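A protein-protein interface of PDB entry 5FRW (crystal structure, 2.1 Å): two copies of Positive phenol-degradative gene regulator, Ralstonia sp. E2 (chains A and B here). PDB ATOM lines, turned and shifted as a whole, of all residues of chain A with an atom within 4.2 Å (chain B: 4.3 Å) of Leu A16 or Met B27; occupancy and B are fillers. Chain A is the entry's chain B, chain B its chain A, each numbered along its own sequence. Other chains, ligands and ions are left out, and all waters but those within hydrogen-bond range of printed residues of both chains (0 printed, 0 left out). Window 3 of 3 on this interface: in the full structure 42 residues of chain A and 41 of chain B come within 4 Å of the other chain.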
ATOM      1  N   ARG A  13      28.938 -31.731 -18.644  1.00  0.00           N
ATOM      2  CA  ARG A  13      28.106 -31.308 -19.752  1.00  0.00           C
ATOM      3  C   ARG A  13      27.305 -32.544 -20.128  1.00  0.00           C
ATOM      4  O   ARG A  13      26.191 -32.451 -20.637  1.00  0.00           O
ATOM      5  CB  ARG A  13      28.968 -30.833 -20.922  1.00  0.00           C
ATOM      6  CG  ARG A  13      29.701 -29.522 -20.659  1.00  0.00           C
ATOM      7  CD  ARG A  13      30.505 -29.083 -21.894  1.00  0.00           C
ATOM      8  NE  ARG A  13      31.280 -27.866 -21.663  1.00  0.00           N
ATOM      9  CZ  ARG A  13      32.144 -27.345 -22.530  1.00  0.00           C
ATOM     10  NH1 ARG A  13      32.364 -27.931 -23.703  1.00  0.00           N
ATOM     11  NH2 ARG A  13      32.799 -26.232 -22.219  1.00  0.00           N
ATOM     12  N   ASP A  14      27.896 -33.706 -19.840  1.00  0.00           N
ATOM     13  CA  ASP A  14      27.287 -35.017 -20.079  1.00  0.00           C
ATOM     14  C   ASP A  14      25.978 -35.186 -19.301  1.00  0.00           C
ATOM     15  O   ASP A  14      25.046 -35.844 -19.756  1.00  0.00           O
ATOM     16  CB  ASP A  14      28.270 -36.134 -19.697  1.00  0.00           C
ATOM     17  CG  ASP A  14      29.447 -36.250 -20.673  1.00  0.00           C
ATOM     18  OD1 ASP A  14      29.380 -35.680 -21.789  1.00  0.00           O
ATOM     19  OD2 ASP A  14      30.440 -36.935 -20.328  1.00  0.00           O
ATOM     20  N   GLY A  15      25.917 -34.585 -18.122  1.00  0.00           N
ATOM     21  CA  GLY A  15      24.712 -34.595 -17.321  1.00  0.00           C
ATOM     22  C   GLY A  15      23.635 -33.719 -17.922  1.00  0.00           C
ATOM     23  O   GLY A  15      22.475 -34.131 -17.966  1.00  0.00           O
ATOM     24  N   LEU A  16      24.011 -32.535 -18.411  1.00  0.00           N
ATOM     25  CA  LEU A  16      23.026 -31.630 -18.983  1.00  0.00           C
ATOM     26  C   LEU A  16      22.350 -32.280 -20.187  1.00  0.00           C
ATOM     27  O   LEU A  16      21.130 -32.398 -20.214  1.00  0.00           O
ATOM     28  CB  LEU A  16      23.660 -30.288 -19.363  1.00  0.00           C
ATOM     29  CG  LEU A  16      24.025 -29.416 -18.156  1.00  0.00           C
ATOM     30  CD1 LEU A  16      24.779 -28.155 -18.575  1.00  0.00           C
ATOM     31  CD2 LEU A  16      22.789 -29.049 -17.333  1.00  0.00           C
ATOM     32  N   SER A  17      23.148 -32.754 -21.140  1.00  0.00           N
ATOM     33  CA  SER A  17      22.614 -33.387 -22.345  1.00  0.00           C
ATOM     34  C   SER A  17      21.794 -34.640 -22.048  1.00  0.00           C
ATOM     35  O   SER A  17      20.771 -34.887 -22.690  1.00  0.00           O
ATOM     36  CB  SER A  17      23.753 -33.723 -23.306  1.00  0.00           C
ATOM     37  OG  SER A  17      24.840 -34.284 -22.596  1.00  0.00           O
ATOM     38  N   ASN A  18      22.214 -35.421 -21.063  1.00  0.00           N
ATOM     39  CA  ASN A  18      21.468 -36.631 -20.736  1.00  0.00           C
ATOM     40  C   ASN A  18      20.242 -36.392 -19.855  1.00  0.00           C
ATOM     41  O   ASN A  18      19.238 -37.092 -19.983  1.00  0.00           O
ATOM     42  CB  ASN A  18      22.380 -37.659 -20.075  1.00  0.00           C
ATOM     43  CG  ASN A  18      22.901 -38.687 -21.062  1.00  0.00           C
ATOM     44  OD1 ASN A  18      22.126 -39.327 -21.777  1.00  0.00           O
ATOM     45  ND2 ASN A  18      24.221 -38.851 -21.107  1.00  0.00           N
ATOM     46  N   LEU A  19      20.304 -35.421 -18.955  1.00  0.00           N
ATOM     47  CA  LEU A  19      19.112 -35.127 -18.173  1.00  0.00           C
ATOM     48  C   LEU A  19      18.123 -34.312 -19.003  1.00  0.00           C
ATOM     49  O   LEU A  19      16.915 -34.501 -18.871  1.00  0.00           O
ATOM     50  CB  LEU A  19      19.463 -34.406 -16.876  1.00  0.00           C
ATOM     51  CG  LEU A  19      19.976 -35.313 -15.757  1.00  0.00           C
ATOM     52  CD1 LEU A  19      20.703 -34.489 -14.706  1.00  0.00           C
ATOM     53  CD2 LEU A  19      18.832 -36.081 -15.132  1.00  0.00           C
ATOM     54  N   ALA A  20      18.628 -33.438 -19.879  1.00  0.00           N
ATOM     55  CA  ALA A  20      17.760 -32.568 -20.693  1.00  0.00           C
ATOM     56  C   ALA A  20      16.866 -33.379 -21.629  1.00  0.00           C
ATOM     57  O   ALA A  20      15.798 -32.911 -22.032  1.00  0.00           O
ATOM     58  CB  ALA A  20      18.582 -31.569 -21.490  1.00  0.00           C
ATOM     59  N   CYS A 100      22.658 -30.122 -12.133  1.00  0.00           N
ATOM     60  CA  CYS A 100      22.237 -30.114 -13.526  1.00  0.00           C
ATOM     61  C   CYS A 100      20.741 -29.825 -13.682  1.00  0.00           C
ATOM     62  O   CYS A 100      20.362 -29.033 -14.522  1.00  0.00           O
ATOM     63  CB  CYS A 100      22.585 -31.442 -14.211  1.00  0.00           C
ATOM     64  SG  CYS A 100      24.355 -31.643 -14.449  1.00  0.00           S
ATOM     65  N   THR A 103      19.902 -26.211 -12.953  1.00  0.00           N
ATOM     66  CA  THR A 103      20.329 -25.425 -14.106  1.00  0.00           C
ATOM     67  C   THR A 103      19.355 -25.571 -15.269  1.00  0.00           C
ATOM     68  O   THR A 103      18.961 -24.591 -15.893  1.00  0.00           O
ATOM     69  CB  THR A 103      21.761 -25.849 -14.572  1.00  0.00           C
ATOM     70  OG1 THR A 103      22.672 -25.752 -13.469  1.00  0.00           O
ATOM     71  CG2 THR A 103      22.244 -24.953 -15.698  1.00  0.00           C
ATOM     72  N   ILE A 104      18.977 -26.803 -15.576  1.00  0.00           N
ATOM     73  CA  ILE A 104      18.043 -27.020 -16.680  1.00  0.00           C
ATOM     74  C   ILE A 104      16.689 -26.323 -16.415  1.00  0.00           C
ATOM     75  O   ILE A 104      16.056 -25.782 -17.322  1.00  0.00           O
ATOM     76  CB  ILE A 104      17.860 -28.536 -16.922  1.00  0.00           C
ATOM     77  CG1 ILE A 104      19.126 -29.110 -17.571  1.00  0.00           C
ATOM     78  CG2 ILE A 104      16.694 -28.810 -17.823  1.00  0.00           C
ATOM     79  CD1 ILE A 104      19.247 -30.648 -17.494  1.00  0.00           C
ATOM     80  N   PHE B  25      15.840 -21.626 -24.119  1.00  0.00           N
ATOM     81  CA  PHE B  25      16.474 -22.409 -23.075  1.00  0.00           C
ATOM     82  C   PHE B  25      17.985 -22.277 -23.147  1.00  0.00           C
ATOM     83  O   PHE B  25      18.595 -22.718 -24.117  1.00  0.00           O
ATOM     84  CB  PHE B  25      16.109 -23.882 -23.208  1.00  0.00           C
ATOM     85  CG  PHE B  25      14.690 -24.203 -22.840  1.00  0.00           C
ATOM     86  CD1 PHE B  25      13.662 -24.048 -23.758  1.00  0.00           C
ATOM     87  CD2 PHE B  25      14.385 -24.688 -21.579  1.00  0.00           C
ATOM     88  CE1 PHE B  25      12.355 -24.357 -23.420  1.00  0.00           C
ATOM     89  CE2 PHE B  25      13.070 -25.002 -21.236  1.00  0.00           C
ATOM     90  CZ  PHE B  25      12.062 -24.835 -22.154  1.00  0.00           C
ATOM     91  N   ALA B  26      18.596 -21.697 -22.118  1.00  0.00           N
ATOM     92  CA  ALA B  26      20.041 -21.501 -22.119  1.00  0.00           C
ATOM     93  C   ALA B  26      20.700 -22.092 -20.876  1.00  0.00           C
ATOM     94  O   ALA B  26      20.910 -21.401 -19.878  1.00  0.00           O
ATOM     95  CB  ALA B  26      20.379 -20.021 -22.238  1.00  0.00           C
ATOM     96  N   MET B  27      21.041 -23.370 -20.955  1.00  0.00           N
ATOM     97  CA  MET B  27      21.726 -24.058 -19.860  1.00  0.00           C
ATOM     98  C   MET B  27      23.206 -23.695 -19.733  1.00  0.00           C
ATOM     99  O   MET B  27      23.929 -24.318 -18.955  1.00  0.00           O
ATOM    100  CB  MET B  27      21.594 -25.555 -20.047  1.00  0.00           C
ATOM    101  CG  MET B  27      20.201 -25.981 -20.413  1.00  0.00           C
ATOM    102  SD  MET B  27      20.219 -27.674 -21.024  1.00  0.00           S
ATOM    103  CE  MET B  27      18.547 -27.801 -21.671  1.00  0.00           C
ATOM    104  N   LYS B  28      23.655 -22.708 -20.511  1.00  0.00           N
ATOM    105  CA  LYS B  28      25.026 -22.200 -20.416  1.00  0.00           C
ATOM    106  C   LYS B  28      25.007 -21.054 -19.443  1.00  0.00           C
ATOM    107  O   LYS B  28      26.034 -20.432 -19.153  1.00  0.00           O
ATOM    108  CB  LYS B  28      25.559 -21.719 -21.766  1.00  0.00           C
ATOM    109  CG  LYS B  28      25.093 -20.319 -22.136  1.00  0.00           C
ATOM    110  CD  LYS B  28      25.770 -19.825 -23.401  1.00  0.00           C
ATOM    111  CE  LYS B  28      25.480 -20.758 -24.571  1.00  0.00           C
ATOM    112  NZ  LYS B  28      26.145 -20.315 -25.834  1.00  0.00           N
ATOM    113  N   GLU B  29      23.808 -20.778 -18.953  1.00  0.00           N
ATOM    114  CA  GLU B  29      23.578 -19.630 -18.113  1.00  0.00           C
ATOM    115  C   GLU B  29      22.538 -20.001 -17.053  1.00  0.00           C
ATOM    116  O   GLU B  29      22.249 -19.221 -16.145  1.00  0.00           O
ATOM    117  CB  GLU B  29      23.166 -18.435 -18.990  1.00  0.00           C
ATOM    118  CG  GLU B  29      24.202 -17.845 -19.953  1.00  0.00           C
ATOM    119  CD  GLU B  29      23.607 -16.720 -20.794  1.00  0.00           C
ATOM    120  OE1 GLU B  29      22.364 -16.556 -20.747  1.00  0.00           O
ATOM    121  OE2 GLU B  29      24.362 -15.998 -21.501  1.00  0.00           O
ATOM    122  N   GLY B  30      22.025 -21.228 -17.148  1.00  0.00           N
ATOM    123  CA  GLY B  30      20.990 -21.704 -16.240  1.00  0.00           C
ATOM    124  C   GLY B  30      19.744 -20.822 -16.246  1.00  0.00           C
ATOM    125  O   GLY B  30      19.165 -20.531 -15.197  1.00  0.00           O
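No position is printed for both chains.
Of the 5 pairs that touch across the chains among the printed residues, none has its exchanged pair printed and touching as well.
Met B27 touches Leu A16.
CB of Ala A20 touches CE of Met B27, at 3.8 Å.
O of Met B27 touches CG2 of Thr A103, 3.7 Å away.
Gly B30 touches Thr A103.
SD of Met B27 touches CG1 of Ile A104, at 3.9 Å.
Of chain B, only Met B27 (3.9 Å) comes within 4 Å of Leu A16.
Of the printed residues of chain B, Ala A20 touches Met B27 (3.8 Å).
Of chain A, only Leu A16 (3.9 Å), Ala A20 (3.8 Å), Thr A103 (3.7 Å) and Ile A104 (3.9 Å) come within 4 Å of Met B27.
Of the printed residues of chain A, Gly B30 touches Thr A103.
The nearest printed residue of chain B that does not touch Ile A104 is Phe B25 (4.7 Å).
Of the 6 printed residues of chain B, 2 touch a printed residue of chain A.
Along chain B the printed residues that touch a printed residue of chain A span positions 27 to 30.
Of the 11 printed residues of chain A, 4 touch a printed residue of chain B.
Printed residues of chain A that touch a printed residue of chain B: Leu A16, Ala A20, Thr A103 and Ile A104.
Among the printed residues, 5 pairs touch across the chains.
Among the printed residues, no Asp or Glu carboxylate lies within 4 Å of a Lys or Arg side-chain nitrogen of the other chain.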
